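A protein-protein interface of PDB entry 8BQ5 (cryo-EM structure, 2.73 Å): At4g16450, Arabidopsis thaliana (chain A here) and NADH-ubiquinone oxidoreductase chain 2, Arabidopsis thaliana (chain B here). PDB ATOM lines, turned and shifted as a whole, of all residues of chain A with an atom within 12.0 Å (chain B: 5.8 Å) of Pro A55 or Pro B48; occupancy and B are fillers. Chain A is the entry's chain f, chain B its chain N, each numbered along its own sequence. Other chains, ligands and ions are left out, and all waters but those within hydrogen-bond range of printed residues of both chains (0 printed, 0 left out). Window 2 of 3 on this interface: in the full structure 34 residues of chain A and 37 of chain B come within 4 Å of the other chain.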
ATOM      1  N   THR A  46     -16.976 -34.839   1.378  1.00  0.00           N
ATOM      2  CA  THR A  46     -17.595 -34.247   0.197  1.00  0.00           C
ATOM      3  C   THR A  46     -18.032 -32.810   0.459  1.00  0.00           C
ATOM      4  O   THR A  46     -17.794 -31.918  -0.367  1.00  0.00           O
ATOM      5  CB  THR A  46     -18.788 -35.096  -0.246  1.00  0.00           C
ATOM      6  OG1 THR A  46     -18.318 -36.320  -0.821  1.00  0.00           O
ATOM      7  CG2 THR A  46     -19.634 -34.351  -1.268  1.00  0.00           C
ATOM      8  N   VAL A  47     -18.679 -32.569   1.602  1.00  0.00           N
ATOM      9  CA  VAL A  47     -19.132 -31.219   1.930  1.00  0.00           C
ATOM     10  C   VAL A  47     -17.940 -30.290   2.111  1.00  0.00           C
ATOM     11  O   VAL A  47     -17.970 -29.129   1.689  1.00  0.00           O
ATOM     12  CB  VAL A  47     -20.036 -31.239   3.177  1.00  0.00           C
ATOM     13  CG1 VAL A  47     -20.345 -29.820   3.635  1.00  0.00           C
ATOM     14  CG2 VAL A  47     -21.325 -31.989   2.882  1.00  0.00           C
ATOM     15  N   GLY A  48     -16.869 -30.786   2.734  1.00  0.00           N
ATOM     16  CA  GLY A  48     -15.670 -29.976   2.865  1.00  0.00           C
ATOM     17  C   GLY A  48     -15.099 -29.575   1.519  1.00  0.00           C
ATOM     18  O   GLY A  48     -14.760 -28.411   1.296  1.00  0.00           O
ATOM     19  N   TYR A  49     -15.004 -30.535   0.596  1.00  0.00           N
ATOM     20  CA  TYR A  49     -14.487 -30.234  -0.736  1.00  0.00           C
ATOM     21  C   TYR A  49     -15.360 -29.213  -1.454  1.00  0.00           C
ATOM     22  O   TYR A  49     -14.860 -28.215  -1.984  1.00  0.00           O
ATOM     23  CB  TYR A  49     -14.387 -31.510  -1.570  1.00  0.00           C
ATOM     24  CG  TYR A  49     -13.912 -31.265  -2.984  1.00  0.00           C
ATOM     25  CD1 TYR A  49     -12.561 -31.142  -3.272  1.00  0.00           C
ATOM     26  CD2 TYR A  49     -14.818 -31.152  -4.031  1.00  0.00           C
ATOM     27  CE1 TYR A  49     -12.125 -30.920  -4.562  1.00  0.00           C
ATOM     28  CE2 TYR A  49     -14.393 -30.926  -5.322  1.00  0.00           C
ATOM     29  CZ  TYR A  49     -13.046 -30.811  -5.582  1.00  0.00           C
ATOM     30  OH  TYR A  49     -12.624 -30.587  -6.870  1.00  0.00           O
ATOM     31  N   LEU A  50     -16.672 -29.454  -1.491  1.00  0.00           N
ATOM     32  CA  LEU A  50     -17.557 -28.594  -2.271  1.00  0.00           C
ATOM     33  C   LEU A  50     -17.649 -27.195  -1.675  1.00  0.00           C
ATOM     34  O   LEU A  50     -17.732 -26.207  -2.413  1.00  0.00           O
ATOM     35  CB  LEU A  50     -18.944 -29.222  -2.384  1.00  0.00           C
ATOM     36  CG  LEU A  50     -19.057 -30.484  -3.238  1.00  0.00           C
ATOM     37  CD1 LEU A  50     -20.479 -31.010  -3.213  1.00  0.00           C
ATOM     38  CD2 LEU A  50     -18.610 -30.207  -4.663  1.00  0.00           C
ATOM     39  N   SER A  51     -17.648 -27.088  -0.346  1.00  0.00           N
ATOM     40  CA  SER A  51     -17.726 -25.778   0.286  1.00  0.00           C
ATOM     41  C   SER A  51     -16.398 -25.035   0.246  1.00  0.00           C
ATOM     42  O   SER A  51     -16.375 -23.822   0.481  1.00  0.00           O
ATOM     43  CB  SER A  51     -18.198 -25.919   1.734  1.00  0.00           C
ATOM     44  OG  SER A  51     -17.272 -26.664   2.503  1.00  0.00           O
ATOM     45  N   GLY A  52     -15.297 -25.725  -0.044  1.00  0.00           N
ATOM     46  CA  GLY A  52     -13.990 -25.101  -0.051  1.00  0.00           C
ATOM     47  C   GLY A  52     -13.499 -24.603  -1.389  1.00  0.00           C
ATOM     48  O   GLY A  52     -12.428 -23.996  -1.454  1.00  0.00           O
ATOM     49  N   ILE A  53     -14.254 -24.837  -2.464  1.00  0.00           N
ATOM     50  CA  ILE A  53     -13.788 -24.465  -3.797  1.00  0.00           C
ATOM     51  C   ILE A  53     -13.746 -22.950  -3.953  1.00  0.00           C
ATOM     52  O   ILE A  53     -12.765 -22.390  -4.455  1.00  0.00           O
ATOM     53  CB  ILE A  53     -14.671 -25.119  -4.876  1.00  0.00           C
ATOM     54  CG1 ILE A  53     -14.306 -26.593  -5.043  1.00  0.00           C
ATOM     55  CG2 ILE A  53     -14.523 -24.393  -6.204  1.00  0.00           C
ATOM     56  CD1 ILE A  53     -15.318 -27.374  -5.838  1.00  0.00           C
ATOM     57  N   LYS A  54     -14.812 -22.262  -3.537  1.00  0.00           N
ATOM     58  CA  LYS A  54     -14.867 -20.812  -3.713  1.00  0.00           C
ATOM     59  C   LYS A  54     -13.756 -20.079  -2.969  1.00  0.00           C
ATOM     60  O   LYS A  54     -13.128 -19.191  -3.571  1.00  0.00           O
ATOM     61  CB  LYS A  54     -16.249 -20.287  -3.310  1.00  0.00           C
ATOM     62  CG  LYS A  54     -16.343 -18.772  -3.323  1.00  0.00           C
ATOM     63  CD  LYS A  54     -17.762 -18.290  -3.104  1.00  0.00           C
ATOM     64  CE  LYS A  54     -18.211 -18.537  -1.677  1.00  0.00           C
ATOM     65  NZ  LYS A  54     -19.691 -18.472  -1.543  1.00  0.00           N
ATOM     66  N   PRO A  55     -13.465 -20.364  -1.693  1.00  0.00           N
ATOM     67  CA  PRO A  55     -12.314 -19.705  -1.056  1.00  0.00           C
ATOM     68  C   PRO A  55     -10.966 -20.161  -1.590  1.00  0.00           C
ATOM     69  O   PRO A  55      -9.966 -19.479  -1.337  1.00  0.00           O
ATOM     70  CB  PRO A  55     -12.476 -20.063   0.427  1.00  0.00           C
ATOM     71  CG  PRO A  55     -13.293 -21.285   0.433  1.00  0.00           C
ATOM     72  CD  PRO A  55     -14.246 -21.135  -0.709  1.00  0.00           C
ATOM     73  N   GLY A  56     -10.895 -21.277  -2.310  1.00  0.00           N
ATOM     74  CA  GLY A  56      -9.633 -21.745  -2.849  1.00  0.00           C
ATOM     75  C   GLY A  56      -8.856 -22.691  -1.965  1.00  0.00           C
ATOM     76  O   GLY A  56      -7.645 -22.843  -2.157  1.00  0.00           O
ATOM     77  N   ILE A  57      -9.510 -23.334  -1.001  1.00  0.00           N
ATOM     78  CA  ILE A  57      -8.847 -24.179  -0.014  1.00  0.00           C
ATOM     79  C   ILE A  57      -9.486 -25.563   0.016  1.00  0.00           C
ATOM     80  O   ILE A  57      -9.636 -26.156   1.088  1.00  0.00           O
ATOM     81  CB  ILE A  57      -8.875 -23.529   1.380  1.00  0.00           C
ATOM     82  CG1 ILE A  57     -10.294 -23.086   1.733  1.00  0.00           C
ATOM     83  CG2 ILE A  57      -7.921 -22.352   1.435  1.00  0.00           C
ATOM     84  CD1 ILE A  57     -10.563 -23.040   3.217  1.00  0.00           C
ATOM     85  N   LYS A  58      -9.918 -26.061  -1.147  1.00  0.00           N
ATOM     86  CA  LYS A  58     -10.658 -27.322  -1.193  1.00  0.00           C
ATOM     87  C   LYS A  58      -9.913 -28.463  -0.500  1.00  0.00           C
ATOM     88  O   LYS A  58     -10.548 -29.323   0.117  1.00  0.00           O
ATOM     89  CB  LYS A  58     -10.981 -27.697  -2.641  1.00  0.00           C
ATOM     90  CG  LYS A  58      -9.773 -27.860  -3.544  1.00  0.00           C
ATOM     91  CD  LYS A  58     -10.189 -27.928  -5.003  1.00  0.00           C
ATOM     92  CE  LYS A  58      -9.422 -29.006  -5.744  1.00  0.00           C
ATOM     93  NZ  LYS A  58      -9.072 -28.575  -7.122  1.00  0.00           N
ATOM     94  N   GLY A  59      -8.585 -28.487  -0.571  1.00  0.00           N
ATOM     95  CA  GLY A  59      -7.811 -29.508   0.102  1.00  0.00           C
ATOM     96  C   GLY A  59      -7.901 -29.438   1.618  1.00  0.00           C
ATOM     97  O   GLY A  59      -8.335 -30.385   2.291  1.00  0.00           O
ATOM     98  N   PRO A  60      -7.461 -28.312   2.190  1.00  0.00           N
ATOM     99  CA  PRO A  60      -7.604 -28.136   3.644  1.00  0.00           C
ATOM    100  C   PRO A  60      -9.041 -28.223   4.128  1.00  0.00           C
ATOM    101  O   PRO A  60      -9.296 -28.727   5.230  1.00  0.00           O
ATOM    102  CB  PRO A  60      -7.010 -26.742   3.876  1.00  0.00           C
ATOM    103  CG  PRO A  60      -6.034 -26.566   2.769  1.00  0.00           C
ATOM    104  CD  PRO A  60      -6.652 -27.242   1.582  1.00  0.00           C
ATOM    105  N   SER A  61      -9.993 -27.729   3.335  1.00  0.00           N
ATOM    106  CA  SER A  61     -11.396 -27.838   3.716  1.00  0.00           C
ATOM    107  C   SER A  61     -11.844 -29.293   3.737  1.00  0.00           C
ATOM    108  O   SER A  61     -12.623 -29.700   4.608  1.00  0.00           O
ATOM    109  CB  SER A  61     -12.262 -27.014   2.767  1.00  0.00           C
ATOM    110  OG  SER A  61     -13.530 -26.756   3.336  1.00  0.00           O
ATOM    111  N   MET A  62     -11.359 -30.093   2.783  1.00  0.00           N
ATOM    112  CA  MET A  62     -11.603 -31.530   2.820  1.00  0.00           C
ATOM    113  C   MET A  62     -11.039 -32.146   4.088  1.00  0.00           C
ATOM    114  O   MET A  62     -11.670 -33.012   4.697  1.00  0.00           O
ATOM    115  CB  MET A  62     -10.988 -32.205   1.597  1.00  0.00           C
ATOM    116  CG  MET A  62     -11.988 -32.712   0.594  1.00  0.00           C
ATOM    117  SD  MET A  62     -11.253 -33.872  -0.571  1.00  0.00           S
ATOM    118  CE  MET A  62      -9.887 -32.891  -1.177  1.00  0.00           C
ATOM    119  N   VAL A  63      -9.840 -31.724   4.490  1.00  0.00           N
ATOM    120  CA  VAL A  63      -9.241 -32.278   5.704  1.00  0.00           C
ATOM    121  C   VAL A  63     -10.092 -31.946   6.925  1.00  0.00           C
ATOM    122  O   VAL A  63     -10.358 -32.807   7.771  1.00  0.00           O
ATOM    123  CB  VAL A  63      -7.798 -31.775   5.876  1.00  0.00           C
ATOM    124  CG1 VAL A  63      -7.225 -32.271   7.193  1.00  0.00           C
ATOM    125  CG2 VAL A  63      -6.939 -32.220   4.711  1.00  0.00           C
ATOM    126  N   THR A  64     -10.523 -30.688   7.038  1.00  0.00           N
ATOM    127  CA  THR A  64     -11.323 -30.269   8.188  1.00  0.00           C
ATOM    128  C   THR A  64     -12.659 -31.007   8.230  1.00  0.00           C
ATOM    129  O   THR A  64     -13.076 -31.520   9.282  1.00  0.00           O
ATOM    130  CB  THR A  64     -11.533 -28.754   8.138  1.00  0.00           C
ATOM    131  OG1 THR A  64     -10.263 -28.096   8.225  1.00  0.00           O
ATOM    132  CG2 THR A  64     -12.418 -28.291   9.278  1.00  0.00           C
ATOM    133  N   GLY A  65     -13.342 -31.079   7.084  1.00  0.00           N
ATOM    134  CA  GLY A  65     -14.585 -31.825   7.022  1.00  0.00           C
ATOM    135  C   GLY A  65     -14.395 -33.292   7.345  1.00  0.00           C
ATOM    136  O   GLY A  65     -15.220 -33.895   8.031  1.00  0.00           O
ATOM    137  N   PHE B  39      -6.858 -20.274   8.136  1.00  0.00           N
ATOM    138  CA  PHE B  39      -6.861 -20.003   6.704  1.00  0.00           C
ATOM    139  C   PHE B  39      -7.366 -18.616   6.337  1.00  0.00           C
ATOM    140  O   PHE B  39      -7.108 -18.162   5.218  1.00  0.00           O
ATOM    141  CB  PHE B  39      -7.650 -21.091   5.980  1.00  0.00           C
ATOM    142  CG  PHE B  39      -6.967 -22.411   6.029  1.00  0.00           C
ATOM    143  CD1 PHE B  39      -5.857 -22.653   5.239  1.00  0.00           C
ATOM    144  CD2 PHE B  39      -7.369 -23.379   6.926  1.00  0.00           C
ATOM    145  CE1 PHE B  39      -5.194 -23.853   5.310  1.00  0.00           C
ATOM    146  CE2 PHE B  39      -6.708 -24.581   7.003  1.00  0.00           C
ATOM    147  CZ  PHE B  39      -5.618 -24.816   6.197  1.00  0.00           C
ATOM    148  N   SER B  40      -8.043 -17.913   7.246  1.00  0.00           N
ATOM    149  CA  SER B  40      -8.434 -16.542   6.946  1.00  0.00           C
ATOM    150  C   SER B  40      -7.246 -15.591   7.009  1.00  0.00           C
ATOM    151  O   SER B  40      -7.248 -14.555   6.334  1.00  0.00           O
ATOM    152  CB  SER B  40      -9.530 -16.086   7.906  1.00  0.00           C
ATOM    153  OG  SER B  40      -8.980 -15.396   9.010  1.00  0.00           O
ATOM    154  N   THR B  41      -6.230 -15.915   7.804  1.00  0.00           N
ATOM    155  CA  THR B  41      -5.043 -15.081   7.933  1.00  0.00           C
ATOM    156  C   THR B  41      -3.951 -15.453   6.939  1.00  0.00           C
ATOM    157  O   THR B  41      -2.878 -14.843   6.959  1.00  0.00           O
ATOM    158  CB  THR B  41      -4.490 -15.164   9.360  1.00  0.00           C
ATOM    159  OG1 THR B  41      -4.320 -16.536   9.733  1.00  0.00           O
ATOM    160  CG2 THR B  41      -5.436 -14.495  10.337  1.00  0.00           C
ATOM    161  N   SER B  42      -4.205 -16.421   6.064  1.00  0.00           N
ATOM    162  CA  SER B  42      -3.172 -16.981   5.200  1.00  0.00           C
ATOM    163  C   SER B  42      -2.933 -16.062   4.009  1.00  0.00           C
ATOM    164  O   SER B  42      -3.865 -15.733   3.268  1.00  0.00           O
ATOM    165  CB  SER B  42      -3.574 -18.378   4.739  1.00  0.00           C
ATOM    166  OG  SER B  42      -2.536 -18.982   3.990  1.00  0.00           O
ATOM    167  N   TYR B  45      -3.336 -18.082   0.426  1.00  0.00           N
ATOM    168  CA  TYR B  45      -4.660 -18.166  -0.168  1.00  0.00           C
ATOM    169  C   TYR B  45      -5.334 -16.806  -0.284  1.00  0.00           C
ATOM    170  O   TYR B  45      -6.549 -16.745  -0.501  1.00  0.00           O
ATOM    171  CB  TYR B  45      -5.532 -19.123   0.642  1.00  0.00           C
ATOM    172  CG  TYR B  45      -4.997 -20.535   0.686  1.00  0.00           C
ATOM    173  CD1 TYR B  45      -4.986 -21.331  -0.450  1.00  0.00           C
ATOM    174  CD2 TYR B  45      -4.503 -21.072   1.866  1.00  0.00           C
ATOM    175  CE1 TYR B  45      -4.501 -22.619  -0.412  1.00  0.00           C
ATOM    176  CE2 TYR B  45      -4.016 -22.359   1.913  1.00  0.00           C
ATOM    177  CZ  TYR B  45      -4.018 -23.129   0.771  1.00  0.00           C
ATOM    178  OH  TYR B  45      -3.533 -24.414   0.812  1.00  0.00           O
ATOM    179  N   ASP B  46      -4.570 -15.721  -0.132  1.00  0.00           N
ATOM    180  CA  ASP B  46      -5.041 -14.352  -0.337  1.00  0.00           C
ATOM    181  C   ASP B  46      -6.155 -13.978   0.641  1.00  0.00           C
ATOM    182  O   ASP B  46      -7.077 -13.239   0.294  1.00  0.00           O
ATOM    183  CB  ASP B  46      -5.490 -14.129  -1.784  1.00  0.00           C
ATOM    184  CG  ASP B  46      -4.328 -14.102  -2.757  1.00  0.00           C
ATOM    185  OD1 ASP B  46      -3.171 -13.971  -2.306  1.00  0.00           O
ATOM    186  OD2 ASP B  46      -4.574 -14.221  -3.976  1.00  0.00           O
ATOM    187  N   TYR B  47      -6.055 -14.474   1.872  1.00  0.00           N
ATOM    188  CA  TYR B  47      -7.003 -14.160   2.935  1.00  0.00           C
ATOM    189  C   TYR B  47      -8.447 -14.381   2.480  1.00  0.00           C
ATOM    190  O   TYR B  47      -9.223 -13.426   2.372  1.00  0.00           O
ATOM    191  CB  TYR B  47      -6.807 -12.736   3.437  1.00  0.00           C
ATOM    192  CG  TYR B  47      -5.364 -12.347   3.652  1.00  0.00           C
ATOM    193  CD1 TYR B  47      -4.734 -12.594   4.863  1.00  0.00           C
ATOM    194  CD2 TYR B  47      -4.636 -11.722   2.650  1.00  0.00           C
ATOM    195  CE1 TYR B  47      -3.418 -12.238   5.068  1.00  0.00           C
ATOM    196  CE2 TYR B  47      -3.319 -11.364   2.846  1.00  0.00           C
ATOM    197  CZ  TYR B  47      -2.716 -11.624   4.056  1.00  0.00           C
ATOM    198  OH  TYR B  47      -1.404 -11.268   4.259  1.00  0.00           O
ATOM    199  N   PRO B  48      -8.833 -15.621   2.203  1.00  0.00           N
ATOM    200  CA  PRO B  48     -10.148 -15.877   1.637  1.00  0.00           C
ATOM    201  C   PRO B  48     -11.243 -15.684   2.669  1.00  0.00           C
ATOM    202  O   PRO B  48     -11.065 -16.010   3.852  1.00  0.00           O
ATOM    203  CB  PRO B  48     -10.052 -17.340   1.194  1.00  0.00           C
ATOM    204  CG  PRO B  48      -9.113 -17.950   2.175  1.00  0.00           C
ATOM    205  CD  PRO B  48      -8.155 -16.865   2.605  1.00  0.00           C
ATOM    206  N   PRO B  49     -12.383 -15.133   2.264  1.00  0.00           N
ATOM    207  CA  PRO B  49     -13.563 -15.172   3.132  1.00  0.00           C
ATOM    208  C   PRO B  49     -13.969 -16.613   3.389  1.00  0.00           C
ATOM    209  O   PRO B  49     -13.998 -17.438   2.474  1.00  0.00           O
ATOM    210  CB  PRO B  49     -14.623 -14.416   2.322  1.00  0.00           C
ATOM    211  CG  PRO B  49     -13.849 -13.611   1.333  1.00  0.00           C
ATOM    212  CD  PRO B  49     -12.655 -14.441   0.996  1.00  0.00           C
ATOM    213  N   LEU B  50     -14.285 -16.918   4.645  1.00  0.00           N
ATOM    214  CA  LEU B  50     -14.618 -18.283   5.027  1.00  0.00           C
ATOM    215  C   LEU B  50     -15.968 -18.393   5.715  1.00  0.00           C
ATOM    216  O   LEU B  50     -16.251 -19.427   6.326  1.00  0.00           O
ATOM    217  CB  LEU B  50     -13.534 -18.867   5.936  1.00  0.00           C
ATOM    218  CG  LEU B  50     -12.126 -19.002   5.362  1.00  0.00           C
ATOM    219  CD1 LEU B  50     -11.218 -19.649   6.389  1.00  0.00           C
ATOM    220  CD2 LEU B  50     -12.143 -19.798   4.072  1.00  0.00           C
ATOM    221  N   ASN B  53     -17.844 -21.235   3.798  1.00  0.00           N
ATOM    222  CA  ASN B  53     -17.185 -22.523   4.017  1.00  0.00           C
ATOM    223  C   ASN B  53     -17.425 -23.031   5.437  1.00  0.00           C
ATOM    224  O   ASN B  53     -17.887 -24.165   5.644  1.00  0.00           O
ATOM    225  CB  ASN B  53     -15.690 -22.377   3.727  1.00  0.00           C
ATOM    226  CG  ASN B  53     -14.905 -23.641   4.003  1.00  0.00           C
ATOM    227  OD1 ASN B  53     -13.990 -23.640   4.823  1.00  0.00           O
ATOM    228  ND2 ASN B  53     -15.257 -24.725   3.326  1.00  0.00           N
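ND2 of Asn B53 lies within hydrogen-bond range of OG of Ser A51, at 2.9 Å. The side-chain hydroxyl of Ser A61 sits at hydrogen-bond distance from the side-chain amide nitrogen of Asn B53 (2.7 Å).
The backbone carbonyl oxygen of Gly A48 is in hydrogen-bond range of the side-chain hydroxyl of Ser A51, 3.3 Å away. O of Gly A48 is in hydrogen-bond range of OG of Ser A61 (2.9 Å). The backbone NH of Ile A57 sits at hydrogen-bond distance from the backbone carbonyl oxygen of Gly A52 (3.0 Å). The backbone NH (N) of Lys A58 lies within hydrogen-bond range of the backbone carbonyl oxygen (O) of Gly A52, at 3.3 Å. O of Val A47 lies within hydrogen-bond range of OG of Ser A51 (2.7 Å). The side-chain hydroxyl of Thr A64 lies within hydrogen-bond range of the backbone carbonyl oxygen of Pro A60, 3.2 Å away.
Among the printed residues, pairs that only touch across the chains: Gly A52 with Asn B53 (3.5 Å), Pro A55 with Pro B48 (3.3 Å), Pro A55 with Pro B49 (3.7 Å), Pro A55 with Leu B50 (3.7 Å), Gly A56 with Tyr B45 (3.5 Å), Ile A57 with Tyr B45 (3.5 Å), Ile A57 with Leu B50 (3.7 Å), Ile A57 with Asn B53 (3.8 Å), Pro A60 with Phe B39 (3.3 Å) and Pro A60 with Tyr B45 (3.8 Å).
Pro B48 touches one residue of chain A. No residue of chain A comes within 4 Å of Ser B40. No residue of chain A comes within 4 Å of Ser B42. No residue of chain A comes within 4 Å of Asp B46. Leu B50 touches just these residues of chain A: Pro A55 (3.7 Å) and Ile A57 (3.7 Å). Of the printed residues of chain B, Ile A57 touches Tyr B45, Leu B50 and Asn B53. Of the printed residues of chain B, Gly A52 touches Asn B53 (3.5 Å). Printed residues of chain A within 4 Å of Tyr B45: Gly A56, Ile A57 and Pro A60. Gly A65 touches none of the printed residues of chain B. The nearest residue of chain B that does not touch Pro A55 is Asn B53 (4.2 Å). The nearest printed residue of chain A that does not touch Tyr B45 is Pro A55 (4.5 Å).
Of the 20 printed residues of chain A, 7 touch a printed residue of chain B. Hydrophobic or aromatic side chains of chain A that line the printed part of chain B: Pro A55, Ile A57 and Pro A60. Among the printed residues, 12 pairs touch across the chains.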
